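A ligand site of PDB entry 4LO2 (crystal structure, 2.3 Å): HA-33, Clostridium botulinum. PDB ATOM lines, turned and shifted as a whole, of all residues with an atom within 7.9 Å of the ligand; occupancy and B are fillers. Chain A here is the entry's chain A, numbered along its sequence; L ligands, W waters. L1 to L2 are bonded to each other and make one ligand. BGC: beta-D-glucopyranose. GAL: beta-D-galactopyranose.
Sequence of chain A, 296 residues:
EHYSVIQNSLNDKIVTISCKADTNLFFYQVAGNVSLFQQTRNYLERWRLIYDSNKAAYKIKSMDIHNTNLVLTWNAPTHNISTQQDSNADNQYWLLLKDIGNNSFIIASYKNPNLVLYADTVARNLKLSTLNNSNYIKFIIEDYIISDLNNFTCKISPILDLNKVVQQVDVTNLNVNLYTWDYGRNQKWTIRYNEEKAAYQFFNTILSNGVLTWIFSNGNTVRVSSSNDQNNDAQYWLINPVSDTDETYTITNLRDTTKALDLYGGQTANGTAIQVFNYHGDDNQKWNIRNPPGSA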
ATOM      1  N   ASN A 220      -6.379 -35.761  -1.203  1.00  0.00           N
ATOM      2  CA  ASN A 220      -7.119 -34.491  -1.247  1.00  0.00           C
ATOM      3  C   ASN A 220      -7.509 -34.048  -2.652  1.00  0.00           C
ATOM      4  O   ASN A 220      -8.042 -32.948  -2.843  1.00  0.00           O
ATOM      5  CB  ASN A 220      -6.286 -33.390  -0.593  1.00  0.00           C
ATOM      6  CG  ASN A 220      -6.086 -33.616   0.899  1.00  0.00           C
ATOM      7  OD1 ASN A 220      -7.019 -33.980   1.613  1.00  0.00           O
ATOM      8  ND2 ASN A 220      -4.876 -33.389   1.368  1.00  0.00           N
ATOM      9  N   ALA A 260     -12.713 -28.625   3.118  1.00  0.00           N
ATOM     10  CA  ALA A 260     -13.077 -27.448   2.345  1.00  0.00           C
ATOM     11  C   ALA A 260     -12.322 -27.379   1.032  1.00  0.00           C
ATOM     12  O   ALA A 260     -11.166 -27.805   0.934  1.00  0.00           O
ATOM     13  CB  ALA A 260     -12.816 -26.188   3.159  1.00  0.00           C
ATOM     14  N   LEU A 261     -13.001 -26.844   0.019  1.00  0.00           N
ATOM     15  CA  LEU A 261     -12.364 -26.514  -1.250  1.00  0.00           C
ATOM     16  C   LEU A 261     -11.241 -25.504  -0.989  1.00  0.00           C
ATOM     17  O   LEU A 261     -11.448 -24.479  -0.346  1.00  0.00           O
ATOM     18  CB  LEU A 261     -13.392 -25.945  -2.241  1.00  0.00           C
ATOM     19  CG  LEU A 261     -12.951 -25.971  -3.715  1.00  0.00           C
ATOM     20  CD1 LEU A 261     -12.762 -27.415  -4.238  1.00  0.00           C
ATOM     21  CD2 LEU A 261     -13.916 -25.190  -4.586  1.00  0.00           C
ATOM     22  N   ASP A 262     -10.056 -25.814  -1.503  1.00  0.00           N
ATOM     23  CA  ASP A 262      -8.812 -25.186  -1.041  1.00  0.00           C
ATOM     24  C   ASP A 262      -7.855 -24.950  -2.214  1.00  0.00           C
ATOM     25  O   ASP A 262      -7.608 -25.844  -3.030  1.00  0.00           O
ATOM     26  CB  ASP A 262      -8.192 -26.092   0.031  1.00  0.00           C
ATOM     27  CG  ASP A 262      -6.827 -25.614   0.533  1.00  0.00           C
ATOM     28  OD1 ASP A 262      -6.766 -25.074   1.664  1.00  0.00           O
ATOM     29  OD2 ASP A 262      -5.822 -25.842  -0.174  1.00  0.00           O
ATOM     30  N   LEU A 263      -7.339 -23.726  -2.311  1.00  0.00           N
ATOM     31  CA  LEU A 263      -6.347 -23.377  -3.313  1.00  0.00           C
ATOM     32  C   LEU A 263      -4.981 -23.732  -2.742  1.00  0.00           C
ATOM     33  O   LEU A 263      -4.560 -23.169  -1.727  1.00  0.00           O
ATOM     34  CB  LEU A 263      -6.425 -21.875  -3.636  1.00  0.00           C
ATOM     35  CG  LEU A 263      -5.405 -21.342  -4.652  1.00  0.00           C
ATOM     36  CD1 LEU A 263      -5.595 -22.044  -5.989  1.00  0.00           C
ATOM     37  CD2 LEU A 263      -5.526 -19.832  -4.823  1.00  0.00           C
ATOM     38  N   TYR A 264      -4.286 -24.666  -3.402  1.00  0.00           N
ATOM     39  CA  TYR A 264      -3.044 -25.244  -2.865  1.00  0.00           C
ATOM     40  C   TYR A 264      -2.005 -24.180  -2.523  1.00  0.00           C
ATOM     41  O   TYR A 264      -1.621 -23.397  -3.381  1.00  0.00           O
ATOM     42  CB  TYR A 264      -2.448 -26.264  -3.842  1.00  0.00           C
ATOM     43  CG  TYR A 264      -1.279 -27.043  -3.259  1.00  0.00           C
ATOM     44  CD1 TYR A 264      -1.478 -28.280  -2.676  1.00  0.00           C
ATOM     45  CD2 TYR A 264       0.018 -26.526  -3.295  1.00  0.00           C
ATOM     46  CE1 TYR A 264      -0.424 -29.002  -2.130  1.00  0.00           C
ATOM     47  CE2 TYR A 264       1.072 -27.234  -2.752  1.00  0.00           C
ATOM     48  CZ  TYR A 264       0.850 -28.466  -2.175  1.00  0.00           C
ATOM     49  OH  TYR A 264       1.911 -29.181  -1.632  1.00  0.00           O
ATOM     50  N   GLY A 265      -1.567 -24.174  -1.270  1.00  0.00           N
ATOM     51  CA  GLY A 265      -0.563 -23.248  -0.797  1.00  0.00           C
ATOM     52  C   GLY A 265      -0.978 -21.783  -0.811  1.00  0.00           C
ATOM     53  O   GLY A 265      -0.256 -20.914  -0.305  1.00  0.00           O
ATOM     54  N   GLY A 266      -2.148 -21.501  -1.368  1.00  0.00           N
ATOM     55  CA  GLY A 266      -2.525 -20.129  -1.664  1.00  0.00           C
ATOM     56  C   GLY A 266      -1.761 -19.547  -2.853  1.00  0.00           C
ATOM     57  O   GLY A 266      -1.707 -18.316  -2.995  1.00  0.00           O
ATOM     58  N   GLN A 267      -1.165 -20.389  -3.694  1.00  0.00           N
ATOM     59  CA  GLN A 267      -0.475 -19.895  -4.886  1.00  0.00           C
ATOM     60  C   GLN A 267      -1.479 -19.512  -5.966  1.00  0.00           C
ATOM     61  O   GLN A 267      -2.585 -20.061  -6.024  1.00  0.00           O
ATOM     62  CB  GLN A 267       0.551 -20.870  -5.471  1.00  0.00           C
ATOM     63  CG  GLN A 267       0.754 -22.178  -4.739  1.00  0.00           C
ATOM     64  CD  GLN A 267       1.960 -22.156  -3.835  1.00  0.00           C
ATOM     65  OE1 GLN A 267       2.417 -21.082  -3.412  1.00  0.00           O
ATOM     66  NE2 GLN A 267       2.499 -23.339  -3.538  1.00  0.00           N
ATOM     67  N   ALA A 273      -3.029 -26.233  -8.290  1.00  0.00           N
ATOM     68  CA  ALA A 273      -4.025 -27.251  -7.967  1.00  0.00           C
ATOM     69  C   ALA A 273      -5.186 -26.732  -7.119  1.00  0.00           C
ATOM     70  O   ALA A 273      -5.008 -25.912  -6.220  1.00  0.00           O
ATOM     71  CB  ALA A 273      -3.359 -28.436  -7.273  1.00  0.00           C
ATOM     72  N   GLN A 275      -7.930 -28.351  -4.554  1.00  0.00           N
ATOM     73  CA  GLN A 275      -8.011 -29.604  -3.806  1.00  0.00           C
ATOM     74  C   GLN A 275      -9.043 -29.432  -2.713  1.00  0.00           C
ATOM     75  O   GLN A 275      -9.759 -28.437  -2.687  1.00  0.00           O
ATOM     76  CB  GLN A 275      -6.656 -29.930  -3.185  1.00  0.00           C
ATOM     77  CG  GLN A 275      -6.228 -28.924  -2.128  1.00  0.00           C
ATOM     78  CD  GLN A 275      -4.850 -29.212  -1.539  1.00  0.00           C
ATOM     79  OE1 GLN A 275      -4.228 -30.218  -1.864  1.00  0.00           O
ATOM     80  NE2 GLN A 275      -4.369 -28.300  -0.683  1.00  0.00           N
ATOM     81  N   VAL A 276      -9.130 -30.428  -1.829  1.00  0.00           N
ATOM     82  CA  VAL A 276      -9.786 -30.227  -0.546  1.00  0.00           C
ATOM     83  C   VAL A 276      -8.707 -30.239   0.523  1.00  0.00           C
ATOM     84  O   VAL A 276      -7.599 -30.736   0.291  1.00  0.00           O
ATOM     85  CB  VAL A 276     -10.848 -31.312  -0.229  1.00  0.00           C
ATOM     86  CG1 VAL A 276     -12.020 -31.200  -1.192  1.00  0.00           C
ATOM     87  CG2 VAL A 276     -10.215 -32.700  -0.250  1.00  0.00           C
ATOM     88  N   PHE A 277      -9.022 -29.680   1.683  1.00  0.00           N
ATOM     89  CA  PHE A 277      -8.067 -29.633   2.777  1.00  0.00           C
ATOM     90  C   PHE A 277      -8.848 -29.344   4.040  1.00  0.00           C
ATOM     91  O   PHE A 277      -9.972 -28.838   3.964  1.00  0.00           O
ATOM     92  CB  PHE A 277      -7.026 -28.530   2.534  1.00  0.00           C
ATOM     93  CG  PHE A 277      -5.777 -28.660   3.372  1.00  0.00           C
ATOM     94  CD1 PHE A 277      -4.745 -29.494   2.959  1.00  0.00           C
ATOM     95  CD2 PHE A 277      -5.644 -27.953   4.565  1.00  0.00           C
ATOM     96  CE1 PHE A 277      -3.590 -29.630   3.723  1.00  0.00           C
ATOM     97  CE2 PHE A 277      -4.494 -28.080   5.339  1.00  0.00           C
ATOM     98  CZ  PHE A 277      -3.457 -28.922   4.917  1.00  0.00           C
ATOM     99  N   ASN A 278      -8.289 -29.680   5.199  1.00  0.00           N
ATOM    100  CA  ASN A 278      -8.953 -29.402   6.472  1.00  0.00           C
ATOM    101  C   ASN A 278      -9.359 -27.933   6.579  1.00  0.00           C
ATOM    102  O   ASN A 278      -8.562 -27.042   6.283  1.00  0.00           O
ATOM    103  CB  ASN A 278      -8.061 -29.801   7.648  1.00  0.00           C
ATOM    104  CG  ASN A 278      -8.683 -29.456   8.984  1.00  0.00           C
ATOM    105  OD1 ASN A 278      -9.720 -30.010   9.357  1.00  0.00           O
ATOM    106  ND2 ASN A 278      -8.061 -28.541   9.709  1.00  0.00           N
ATOM    107  N   TYR A 279     -10.598 -27.686   6.969  1.00  0.00           N
ATOM    108  CA  TYR A 279     -11.119 -26.328   7.013  1.00  0.00           C
ATOM    109  C   TYR A 279     -10.412 -25.496   8.074  1.00  0.00           C
ATOM    110  O   TYR A 279     -10.336 -25.903   9.237  1.00  0.00           O
ATOM    111  CB  TYR A 279     -12.635 -26.322   7.258  1.00  0.00           C
ATOM    112  CG  TYR A 279     -13.202 -24.931   7.430  1.00  0.00           C
ATOM    113  CD1 TYR A 279     -13.543 -24.155   6.324  1.00  0.00           C
ATOM    114  CD2 TYR A 279     -13.381 -24.368   8.697  1.00  0.00           C
ATOM    115  CE1 TYR A 279     -14.045 -22.882   6.470  1.00  0.00           C
ATOM    116  CE2 TYR A 279     -13.881 -23.093   8.853  1.00  0.00           C
ATOM    117  CZ  TYR A 279     -14.218 -22.355   7.731  1.00  0.00           C
ATOM    118  OH  TYR A 279     -14.718 -21.080   7.887  1.00  0.00           O
ATOM    119  N   HIS A 280      -9.892 -24.340   7.668  1.00  0.00           N
ATOM    120  CA  HIS A 280      -9.342 -23.392   8.618  1.00  0.00           C
ATOM    121  C   HIS A 280      -9.872 -21.989   8.347  1.00  0.00           C
ATOM    122  O   HIS A 280      -9.692 -21.078   9.139  1.00  0.00           O
ATOM    123  CB  HIS A 280      -7.800 -23.410   8.617  1.00  0.00           C
ATOM    124  CG  HIS A 280      -7.185 -23.394   7.257  1.00  0.00           C
ATOM    125  ND1 HIS A 280      -7.487 -22.443   6.301  1.00  0.00           N
ATOM    126  CD2 HIS A 280      -6.262 -24.203   6.687  1.00  0.00           C
ATOM    127  CE1 HIS A 280      -6.787 -22.678   5.211  1.00  0.00           C
ATOM    128  NE2 HIS A 280      -6.034 -23.743   5.416  1.00  0.00           N
ATOM    129  N   GLY A 281     -10.559 -21.838   7.211  1.00  0.00           N
ATOM    130  CA  GLY A 281     -11.198 -20.584   6.872  1.00  0.00           C
ATOM    131  C   GLY A 281     -10.250 -19.457   6.520  1.00  0.00           C
ATOM    132  O   GLY A 281     -10.616 -18.285   6.594  1.00  0.00           O
ATOM    133  N   ASP A 282      -9.016 -19.795   6.145  1.00  0.00           N
ATOM    134  CA  ASP A 282      -8.092 -18.784   5.641  1.00  0.00           C
ATOM    135  C   ASP A 282      -8.555 -18.345   4.261  1.00  0.00           C
ATOM    136  O   ASP A 282      -9.516 -18.899   3.691  1.00  0.00           O
ATOM    137  CB  ASP A 282      -6.663 -19.321   5.579  1.00  0.00           C
ATOM    138  CG  ASP A 282      -6.062 -19.566   6.953  1.00  0.00           C
ATOM    139  OD1 ASP A 282      -6.570 -18.953   7.926  1.00  0.00           O
ATOM    140  OD2 ASP A 282      -5.077 -20.341   7.067  1.00  0.00           O
ATOM    141  N   ASN A 284      -7.295 -18.697   1.316  1.00  0.00           N
ATOM    142  CA  ASN A 284      -7.206 -19.697   0.249  1.00  0.00           C
ATOM    143  C   ASN A 284      -8.328 -20.745   0.293  1.00  0.00           C
ATOM    144  O   ASN A 284      -8.339 -21.657  -0.521  1.00  0.00           O
ATOM    145  CB  ASN A 284      -5.823 -20.380   0.218  1.00  0.00           C
ATOM    146  CG  ASN A 284      -5.618 -21.363   1.343  1.00  0.00           C
ATOM    147  OD1 ASN A 284      -5.862 -21.058   2.518  1.00  0.00           O
ATOM    148  ND2 ASN A 284      -5.175 -22.575   1.002  1.00  0.00           N
ATOM    149  N   GLN A 285      -9.259 -20.609   1.237  1.00  0.00           N
ATOM    150  CA  GLN A 285     -10.454 -21.475   1.267  1.00  0.00           C
ATOM    151  C   GLN A 285     -11.736 -20.641   1.099  1.00  0.00           C
ATOM    152  O   GLN A 285     -12.841 -21.078   1.446  1.00  0.00           O
ATOM    153  CB  GLN A 285     -10.523 -22.286   2.562  1.00  0.00           C
ATOM    154  CG  GLN A 285      -9.314 -23.195   2.808  1.00  0.00           C
ATOM    155  CD  GLN A 285      -9.463 -24.097   4.030  1.00  0.00           C
ATOM    156  OE1 GLN A 285     -10.291 -23.855   4.907  1.00  0.00           O
ATOM    157  NE2 GLN A 285      -8.653 -25.141   4.086  1.00  0.00           N
HETATM  158  C2  BGC L   1       3.541 -23.710   2.192  1.00  0.00           C
HETATM  159  C3  BGC L   1       2.150 -23.901   1.979  1.00  0.00           C
HETATM  160  C4  BGC L   1       1.317 -23.847   3.217  1.00  0.00           C
HETATM  161  C5  BGC L   1       1.773 -22.883   4.275  1.00  0.00           C
HETATM  162  C6  BGC L   1       1.268 -23.271   5.672  1.00  0.00           C
HETATM  163  C1  BGC L   1       3.804 -22.521   3.058  1.00  0.00           C
HETATM  164  O1  BGC L   1       5.180 -22.229   3.185  1.00  0.00           O
HETATM  165  O2  BGC L   1       4.154 -23.475   0.953  1.00  0.00           O
HETATM  166  O3  BGC L   1       2.053 -25.178   1.456  1.00  0.00           O
HETATM  167  O4  BGC L   1      -0.028 -23.493   2.868  1.00  0.00           O
HETATM  168  O5  BGC L   1       3.157 -22.708   4.379  1.00  0.00           O
HETATM  169  O6  BGC L   1       0.570 -22.285   6.387  1.00  0.00           O
HETATM  170  C1  GAL L   2      -0.878 -24.612   2.983  1.00  0.00           C
HETATM  171  C2  GAL L   2      -2.306 -24.151   3.202  1.00  0.00           C
HETATM  172  C3  GAL L   2      -3.301 -25.266   3.128  1.00  0.00           C
HETATM  173  C4  GAL L   2      -3.116 -26.111   1.987  1.00  0.00           C
HETATM  174  C5  GAL L   2      -1.704 -26.593   1.909  1.00  0.00           C
HETATM  175  C6  GAL L   2      -1.413 -27.458   0.719  1.00  0.00           C
HETATM  176  O2  GAL L   2      -2.420 -23.536   4.427  1.00  0.00           O
HETATM  177  O3  GAL L   2      -4.591 -24.630   3.116  1.00  0.00           O
HETATM  178  O4  GAL L   2      -3.357 -25.359   0.803  1.00  0.00           O
HETATM  179  O5  GAL L   2      -0.740 -25.464   1.894  1.00  0.00           O
HETATM  180  O6  GAL L   2      -1.983 -28.718   0.729  1.00  0.00           O
HETATM  181  O   HOH W   1      -3.557 -21.119   4.302  1.00  0.00           O
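A ring nitrogen (NE2) of His 280 is in hydrogen-bond range of an oxygen (O3) of GAL L2 (2.9 Å).
The side-chain amide nitrogen (ND2) of Asn 284 lies within hydrogen-bond range of an oxygen (O3) of GAL L2.
The side-chain carboxylate of Asp 262 lies within hydrogen-bond range of an oxygen (O3) of GAL L2.
O6 of GAL L2 sits at hydrogen-bond distance from NE2 of Gln 275.
N of Gly 265 sits at hydrogen-bond distance from O4 of GAL L2.
The backbone carbonyl oxygen (O) of Phe 277 lies within hydrogen-bond range of the backbone NH (N) of Ala 260 (2.9 Å).
The side-chain amide nitrogen (ND2) of Asn 284 lies within hydrogen-bond range of the side-chain carboxylate (OD1) of Asp 262, at 3.0 Å.
The side-chain amide nitrogen of Asn 284 is in hydrogen-bond range of the backbone carbonyl oxygen of Leu 263, at 2.9 Å.
NE2 of Gln 285 sits at hydrogen-bond distance from OD1 of Asp 262 (3.1 Å).
N of Asp 262 sits at hydrogen-bond distance from O of Gln 275, at 2.9 Å.
ND1 of His 280 sits at hydrogen-bond distance from N of Asp 282 (3.1 Å).
The side-chain amide oxygen of Gln 285 sits at hydrogen-bond distance from the backbone NH of His 280 (2.8 Å).
N of Tyr 264 lies within hydrogen-bond range of O of Ala 273 (3.2 Å).
O of Leu 263 touches O4 of GAL L2, at 3.6 Å.
Tyr 264 touches the ligand.
CE1 of Phe 277 touches O6 of GAL L2, 3.5 Å away.
Hydrophobic or aromatic side chains that line the ligand: Tyr 264, Phe 277 and His 280.
Eight residues have an atom within 4 Å of the ligand: Asp 262, Leu 263, Tyr 264, Gly 265, Gln 275, Phe 277, His 280 and Asn 284.
Water W1 lies within hydrogen-bond range of O2 of GAL L2, OD1 of Asn 284 and OD2 of Asp 282.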
